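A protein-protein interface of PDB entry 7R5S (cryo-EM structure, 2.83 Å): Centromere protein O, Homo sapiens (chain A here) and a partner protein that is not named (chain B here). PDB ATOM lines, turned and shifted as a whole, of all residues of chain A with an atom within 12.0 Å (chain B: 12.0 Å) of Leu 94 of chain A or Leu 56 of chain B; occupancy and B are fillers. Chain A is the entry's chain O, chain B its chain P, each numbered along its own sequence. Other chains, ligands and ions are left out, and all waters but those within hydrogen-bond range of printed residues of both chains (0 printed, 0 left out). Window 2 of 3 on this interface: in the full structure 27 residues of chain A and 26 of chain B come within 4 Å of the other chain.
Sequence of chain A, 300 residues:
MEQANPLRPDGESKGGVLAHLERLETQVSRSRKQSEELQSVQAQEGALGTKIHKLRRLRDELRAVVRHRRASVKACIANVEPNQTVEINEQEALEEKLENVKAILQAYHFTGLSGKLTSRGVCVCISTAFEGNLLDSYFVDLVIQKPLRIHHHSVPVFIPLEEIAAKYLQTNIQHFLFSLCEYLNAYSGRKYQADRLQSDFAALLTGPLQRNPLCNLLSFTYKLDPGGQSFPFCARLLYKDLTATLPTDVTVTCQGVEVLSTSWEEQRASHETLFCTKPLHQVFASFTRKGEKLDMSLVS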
ATOM      1  N   ASN A  89      34.246   2.898  -4.744  1.00  0.00           N
ATOM      2  CA  ASN A  89      33.327   3.333  -3.699  1.00  0.00           C
ATOM      3  C   ASN A  89      32.052   3.918  -4.297  1.00  0.00           C
ATOM      4  O   ASN A  89      31.512   3.390  -5.269  1.00  0.00           O
ATOM      5  CB  ASN A  89      34.000   4.359  -2.785  1.00  0.00           C
ATOM      6  N   GLU A  90      31.574   5.016  -3.708  1.00  0.00           N
ATOM      7  CA  GLU A  90      30.357   5.656  -4.194  1.00  0.00           C
ATOM      8  C   GLU A  90      30.561   6.356  -5.531  1.00  0.00           C
ATOM      9  O   GLU A  90      29.583   6.581  -6.253  1.00  0.00           O
ATOM     10  CB  GLU A  90      29.838   6.655  -3.158  1.00  0.00           C
ATOM     11  N   GLN A  91      31.804   6.707  -5.873  1.00  0.00           N
ATOM     12  CA  GLN A  91      32.060   7.389  -7.137  1.00  0.00           C
ATOM     13  C   GLN A  91      31.698   6.506  -8.326  1.00  0.00           C
ATOM     14  O   GLN A  91      31.192   6.997  -9.342  1.00  0.00           O
ATOM     15  CB  GLN A  91      33.525   7.818  -7.214  1.00  0.00           C
ATOM     16  N   GLU A  92      31.944   5.199  -8.214  1.00  0.00           N
ATOM     17  CA  GLU A  92      31.604   4.284  -9.299  1.00  0.00           C
ATOM     18  C   GLU A  92      30.099   4.253  -9.536  1.00  0.00           C
ATOM     19  O   GLU A  92      29.635   4.358 -10.678  1.00  0.00           O
ATOM     20  CB  GLU A  92      32.132   2.883  -8.988  1.00  0.00           C
ATOM     21  N   ALA A  93      29.316   4.115  -8.463  1.00  0.00           N
ATOM     22  CA  ALA A  93      27.863   4.104  -8.604  1.00  0.00           C
ATOM     23  C   ALA A  93      27.338   5.446  -9.095  1.00  0.00           C
ATOM     24  O   ALA A  93      26.376   5.489  -9.872  1.00  0.00           O
ATOM     25  CB  ALA A  93      27.208   3.729  -7.275  1.00  0.00           C
ATOM     26  N   LEU A  94      27.957   6.548  -8.667  1.00  0.00           N
ATOM     27  CA  LEU A  94      27.520   7.861  -9.128  1.00  0.00           C
ATOM     28  C   LEU A  94      27.783   8.040 -10.619  1.00  0.00           C
ATOM     29  O   LEU A  94      26.921   8.540 -11.352  1.00  0.00           O
ATOM     30  CB  LEU A  94      28.214   8.955  -8.317  1.00  0.00           C
ATOM     31  CG  LEU A  94      27.386   9.582  -7.194  1.00  0.00           C
ATOM     32  CD1 LEU A  94      26.941   8.528  -6.193  1.00  0.00           C
ATOM     33  CD2 LEU A  94      28.182  10.669  -6.498  1.00  0.00           C
ATOM     34  N   GLU A  95      28.963   7.625 -11.089  1.00  0.00           N
ATOM     35  CA  GLU A  95      29.247   7.680 -12.518  1.00  0.00           C
ATOM     36  C   GLU A  95      28.336   6.746 -13.303  1.00  0.00           C
ATOM     37  O   GLU A  95      27.940   7.067 -14.430  1.00  0.00           O
ATOM     38  CB  GLU A  95      30.715   7.338 -12.777  1.00  0.00           C
ATOM     39  N   GLU A  96      27.989   5.593 -12.725  1.00  0.00           N
ATOM     40  CA  GLU A  96      27.059   4.683 -13.382  1.00  0.00           C
ATOM     41  C   GLU A  96      25.687   5.327 -13.541  1.00  0.00           C
ATOM     42  O   GLU A  96      25.073   5.253 -14.611  1.00  0.00           O
ATOM     43  CB  GLU A  96      26.957   3.377 -12.593  1.00  0.00           C
ATOM     44  N   LYS A  97      25.192   5.972 -12.482  1.00  0.00           N
ATOM     45  CA  LYS A  97      23.910   6.664 -12.572  1.00  0.00           C
ATOM     46  C   LYS A  97      23.969   7.805 -13.582  1.00  0.00           C
ATOM     47  O   LYS A  97      23.010   8.034 -14.332  1.00  0.00           O
ATOM     48  CB  LYS A  97      23.497   7.186 -11.196  1.00  0.00           C
ATOM     49  CG  LYS A  97      23.184   6.096 -10.184  1.00  0.00           C
ATOM     50  CD  LYS A  97      21.898   5.366 -10.538  1.00  0.00           C
ATOM     51  CE  LYS A  97      20.707   6.310 -10.526  1.00  0.00           C
ATOM     52  NZ  LYS A  97      19.437   5.606 -10.853  1.00  0.00           N
ATOM     53  N   LEU A  98      25.093   8.526 -13.620  1.00  0.00           N
ATOM     54  CA  LEU A  98      25.241   9.624 -14.569  1.00  0.00           C
ATOM     55  C   LEU A  98      25.184   9.122 -16.007  1.00  0.00           C
ATOM     56  O   LEU A  98      24.434   9.654 -16.834  1.00  0.00           O
ATOM     57  CB  LEU A  98      26.551  10.369 -14.307  1.00  0.00           C
ATOM     58  CG  LEU A  98      26.521  11.426 -13.202  1.00  0.00           C
ATOM     59  CD1 LEU A  98      27.906  12.014 -12.984  1.00  0.00           C
ATOM     60  CD2 LEU A  98      25.522  12.521 -13.539  1.00  0.00           C
ATOM     61  N   GLU A  99      25.978   8.096 -16.327  1.00  0.00           N
ATOM     62  CA  GLU A  99      25.953   7.564 -17.686  1.00  0.00           C
ATOM     63  C   GLU A  99      24.606   6.932 -18.012  1.00  0.00           C
ATOM     64  O   GLU A  99      24.162   6.991 -19.164  1.00  0.00           O
ATOM     65  CB  GLU A  99      27.093   6.563 -17.891  1.00  0.00           C
ATOM     66  CG  GLU A  99      27.038   5.323 -17.017  1.00  0.00           C
ATOM     67  CD  GLU A  99      26.288   4.176 -17.668  1.00  0.00           C
ATOM     68  OE1 GLU A  99      26.000   4.262 -18.880  1.00  0.00           O
ATOM     69  OE2 GLU A  99      25.989   3.187 -16.966  1.00  0.00           O
ATOM     70  N   ASN A 100      23.924   6.363 -17.014  1.00  0.00           N
ATOM     71  CA  ASN A 100      22.607   5.783 -17.251  1.00  0.00           C
ATOM     72  C   ASN A 100      21.599   6.856 -17.643  1.00  0.00           C
ATOM     73  O   ASN A 100      20.869   6.706 -18.629  1.00  0.00           O
ATOM     74  CB  ASN A 100      22.138   5.029 -16.006  1.00  0.00           C
ATOM     75  CG  ASN A 100      20.800   4.346 -16.209  1.00  0.00           C
ATOM     76  OD1 ASN A 100      20.430   4.001 -17.330  1.00  0.00           O
ATOM     77  ND2 ASN A 100      20.067   4.148 -15.120  1.00  0.00           N
ATOM     78  N   VAL A 101      21.547   7.954 -16.883  1.00  0.00           N
ATOM     79  CA  VAL A 101      20.587   9.003 -17.215  1.00  0.00           C
ATOM     80  C   VAL A 101      20.976   9.703 -18.515  1.00  0.00           C
ATOM     81  O   VAL A 101      20.103  10.137 -19.277  1.00  0.00           O
ATOM     82  CB  VAL A 101      20.430   9.999 -16.050  1.00  0.00           C
ATOM     83  CG1 VAL A 101      19.956   9.277 -14.797  1.00  0.00           C
ATOM     84  CG2 VAL A 101      21.723  10.746 -15.784  1.00  0.00           C
ATOM     85  N   LYS A 102      22.276   9.795 -18.814  1.00  0.00           N
ATOM     86  CA  LYS A 102      22.688  10.373 -20.090  1.00  0.00           C
ATOM     87  C   LYS A 102      22.236   9.506 -21.260  1.00  0.00           C
ATOM     88  O   LYS A 102      21.728  10.024 -22.263  1.00  0.00           O
ATOM     89  CB  LYS A 102      24.204  10.567 -20.117  1.00  0.00           C
ATOM     90  CG  LYS A 102      24.695  11.725 -19.263  1.00  0.00           C
ATOM     91  CD  LYS A 102      26.205  11.871 -19.346  1.00  0.00           C
ATOM     92  CE  LYS A 102      26.703  12.970 -18.423  1.00  0.00           C
ATOM     93  NZ  LYS A 102      26.394  12.675 -16.997  1.00  0.00           N
ATOM     94  N   ALA A 103      22.414   8.186 -21.152  1.00  0.00           N
ATOM     95  CA  ALA A 103      21.935   7.290 -22.198  1.00  0.00           C
ATOM     96  C   ALA A 103      20.418   7.340 -22.313  1.00  0.00           C
ATOM     97  O   ALA A 103      19.868   7.262 -23.419  1.00  0.00           O
ATOM     98  CB  ALA A 103      22.407   5.862 -21.922  1.00  0.00           C
ATOM     99  N   SER B  53      30.930  15.332  -1.941  1.00  0.00           N
ATOM    100  CA  SER B  53      30.169  14.823  -3.075  1.00  0.00           C
ATOM    101  C   SER B  53      28.755  15.396  -3.088  1.00  0.00           C
ATOM    102  O   SER B  53      27.839  14.801  -3.656  1.00  0.00           O
ATOM    103  CB  SER B  53      30.116  13.294  -3.044  1.00  0.00           C
ATOM    104  OG  SER B  53      31.301  12.732  -3.584  1.00  0.00           O
ATOM    105  N   LYS B  54      28.584  16.559  -2.456  1.00  0.00           N
ATOM    106  CA  LYS B  54      27.273  17.199  -2.432  1.00  0.00           C
ATOM    107  C   LYS B  54      26.903  17.750  -3.803  1.00  0.00           C
ATOM    108  O   LYS B  54      25.732  17.713  -4.199  1.00  0.00           O
ATOM    109  CB  LYS B  54      27.248  18.307  -1.381  1.00  0.00           C
ATOM    110  N   ASP B  55      27.889  18.268  -4.541  1.00  0.00           N
ATOM    111  CA  ASP B  55      27.619  18.769  -5.885  1.00  0.00           C
ATOM    112  C   ASP B  55      27.166  17.648  -6.810  1.00  0.00           C
ATOM    113  O   ASP B  55      26.284  17.845  -7.653  1.00  0.00           O
ATOM    114  CB  ASP B  55      28.862  19.460  -6.447  1.00  0.00           C
ATOM    115  N   LEU B  56      27.750  16.458  -6.659  1.00  0.00           N
ATOM    116  CA  LEU B  56      27.336  15.324  -7.480  1.00  0.00           C
ATOM    117  C   LEU B  56      25.911  14.896  -7.152  1.00  0.00           C
ATOM    118  O   LEU B  56      25.135  14.560  -8.054  1.00  0.00           O
ATOM    119  CB  LEU B  56      28.306  14.160  -7.294  1.00  0.00           C
ATOM    120  N   LYS B  57      25.547  14.905  -5.867  1.00  0.00           N
ATOM    121  CA  LYS B  57      24.175  14.581  -5.489  1.00  0.00           C
ATOM    122  C   LYS B  57      23.198  15.620  -6.024  1.00  0.00           C
ATOM    123  O   LYS B  57      22.098  15.277  -6.476  1.00  0.00           O
ATOM    124  CB  LYS B  57      24.062  14.468  -3.969  1.00  0.00           C
ATOM    125  N   ASN B  58      23.586  16.898  -5.987  1.00  0.00           N
ATOM    126  CA  ASN B  58      22.736  17.943  -6.548  1.00  0.00           C
ATOM    127  C   ASN B  58      22.564  17.764  -8.052  1.00  0.00           C
ATOM    128  O   ASN B  58      21.462  17.946  -8.585  1.00  0.00           O
ATOM    129  CB  ASN B  58      23.321  19.320  -6.234  1.00  0.00           C
ATOM    130  N   GLN B  59      23.642  17.405  -8.752  1.00  0.00           N
ATOM    131  CA  GLN B  59      23.548  17.155 -10.187  1.00  0.00           C
ATOM    132  C   GLN B  59      22.641  15.968 -10.481  1.00  0.00           C
ATOM    133  O   GLN B  59      21.833  16.011 -11.417  1.00  0.00           O
ATOM    134  CB  GLN B  59      24.939  16.926 -10.776  1.00  0.00           C
ATOM    135  CG  GLN B  59      25.553  18.158 -11.421  1.00  0.00           C
ATOM    136  CD  GLN B  59      25.868  19.247 -10.415  1.00  0.00           C
ATOM    137  OE1 GLN B  59      25.131  20.225 -10.290  1.00  0.00           O
ATOM    138  NE2 GLN B  59      26.970  19.084  -9.692  1.00  0.00           N
ATOM    139  N   LEU B  60      22.765  14.894  -9.696  1.00  0.00           N
ATOM    140  CA  LEU B  60      21.894  13.737  -9.876  1.00  0.00           C
ATOM    141  C   LEU B  60      20.432  14.110  -9.661  1.00  0.00           C
ATOM    142  O   LEU B  60      19.559  13.711 -10.443  1.00  0.00           O
ATOM    143  CB  LEU B  60      22.305  12.615  -8.923  1.00  0.00           C
ATOM    144  CG  LEU B  60      23.099  11.452  -9.521  1.00  0.00           C
ATOM    145  CD1 LEU B  60      22.289  10.743 -10.595  1.00  0.00           C
ATOM    146  CD2 LEU B  60      24.428  11.937 -10.077  1.00  0.00           C
ATOM    147  N   GLY B  61      20.149  14.876  -8.605  1.00  0.00           N
ATOM    148  CA  GLY B  61      18.780  15.301  -8.361  1.00  0.00           C
ATOM    149  C   GLY B  61      18.234  16.181  -9.469  1.00  0.00           C
ATOM    150  O   GLY B  61      17.084  16.024  -9.890  1.00  0.00           O
ATOM    151  N   HIS B  62      19.052  17.116  -9.960  1.00  0.00           N
ATOM    152  CA  HIS B  62      18.616  17.983 -11.049  1.00  0.00           C
ATOM    153  C   HIS B  62      18.343  17.185 -12.318  1.00  0.00           C
ATOM    154  O   HIS B  62      17.355  17.437 -13.018  1.00  0.00           O
ATOM    155  CB  HIS B  62      19.667  19.063 -11.313  1.00  0.00           C
ATOM    156  CG  HIS B  62      19.791  20.066 -10.209  1.00  0.00           C
ATOM    157  ND1 HIS B  62      18.947  20.084  -9.119  1.00  0.00           N
ATOM    158  CD2 HIS B  62      20.662  21.088 -10.027  1.00  0.00           C
ATOM    159  CE1 HIS B  62      19.292  21.073  -8.315  1.00  0.00           C
ATOM    160  NE2 HIS B  62      20.329  21.698  -8.841  1.00  0.00           N
ATOM    161  N   LEU B  63      19.204  16.212 -12.627  1.00  0.00           N
ATOM    162  CA  LEU B  63      18.993  15.399 -13.820  1.00  0.00           C
ATOM    163  C   LEU B  63      17.744  14.537 -13.687  1.00  0.00           C
ATOM    164  O   LEU B  63      16.988  14.382 -14.652  1.00  0.00           O
ATOM    165  CB  LEU B  63      20.221  14.532 -14.093  1.00  0.00           C
ATOM    166  CG  LEU B  63      21.460  15.273 -14.601  1.00  0.00           C
ATOM    167  CD1 LEU B  63      22.567  14.294 -14.955  1.00  0.00           C
ATOM    168  CD2 LEU B  63      21.110  16.146 -15.797  1.00  0.00           C
ATOM    169  N   GLU B  64      17.500  13.978 -12.498  1.00  0.00           N
ATOM    170  CA  GLU B  64      16.287  13.194 -12.294  1.00  0.00           C
ATOM    171  C   GLU B  64      15.041  14.064 -12.416  1.00  0.00           C
ATOM    172  O   GLU B  64      14.037  13.644 -13.009  1.00  0.00           O
ATOM    173  CB  GLU B  64      16.330  12.503 -10.931  1.00  0.00           C
ATOM    174  CG  GLU B  64      17.336  11.367 -10.841  1.00  0.00           C
ATOM    175  CD  GLU B  64      16.904  10.137 -11.615  1.00  0.00           C
ATOM    176  OE1 GLU B  64      15.696  10.006 -11.904  1.00  0.00           O
ATOM    177  OE2 GLU B  64      17.774   9.299 -11.937  1.00  0.00           O
ATOM    178  N   SER B  65      15.089  15.283 -11.872  1.00  0.00           N
ATOM    179  CA  SER B  65      13.949  16.187 -11.984  1.00  0.00           C
ATOM    180  C   SER B  65      13.695  16.577 -13.434  1.00  0.00           C
ATOM    181  O   SER B  65      12.543  16.626 -13.878  1.00  0.00           O
ATOM    182  CB  SER B  65      14.178  17.430 -11.125  1.00  0.00           C
ATOM    183  OG  SER B  65      14.895  18.420 -11.842  1.00  0.00           O
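Leu 94 of chain A touches just one residue of chain B: Leu 56 (3.6 Å). Of chain A, only Leu 94 (3.6 Å) comes within 4 Å of Leu 56 of chain B. No residue of chain B comes within 4 Å of Glu 90 of chain A. No residue of chain B comes within 4 Å of Glu 92 of chain A. No residue of chain B comes within 4 Å of Ala 93 of chain A. Glu 95 of chain A touches none of the printed residues of chain B. Of chain B, only Leu 60 and Leu 63 come within 4 Å of Leu 98 of chain A. No residue of chain A comes within 4 Å of Ser 53 of chain B. No residue of chain A comes within 4 Å of Lys 54 of chain B. No residue of chain A comes within 4 Å of Asp 55 of chain B. No residue of chain A comes within 4 Å of Lys 57 of chain B. No residue of chain A comes within 4 Å of Asn 58 of chain B. Printed residues of chain A within 4 Å of Glu 64 of chain B: Val 101 (3.6 Å). Of the printed residues of chain B, Val 101 of chain A touches Leu 63 (3.7 Å) and Glu 64 (3.6 Å). Printed residues of chain B within 4 Å of Lys 97 of chain A: Leu 60 (3.8 Å). The nearest printed residue of chain A that does not touch Leu 63 of chain B is Lys 102 of chain A (4.6 Å).
Printed residues of chain B that touch a printed residue of chain A: Leu 56, Leu 60, Leu 63 and Glu 64. Of the 15 printed residues of chain A, 4 touch a printed residue of chain B. Printed residues of chain A that touch a printed residue of chain B: Leu 94, Lys 97, Leu 98 and Val 101. Hydrophobic or aromatic side chains of chain A within 4 Å of the printed part of chain B: Leu 94, Leu 98 and Val 101. Among the printed residues, 6 pairs touch across the chains.
Among the printed residues, pairs that only touch across the chains: Leu 94 of chain A with Leu 56 of chain B, Val 101 of chain A with Glu 64 of chain B, Leu 98 of chain A with Leu 60 of chain B, Leu 98 of chain A with Leu 63 of chain B, Val 101 of chain A with Leu 63 of chain B and Lys 97 of chain A with Leu 60 of chain B.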
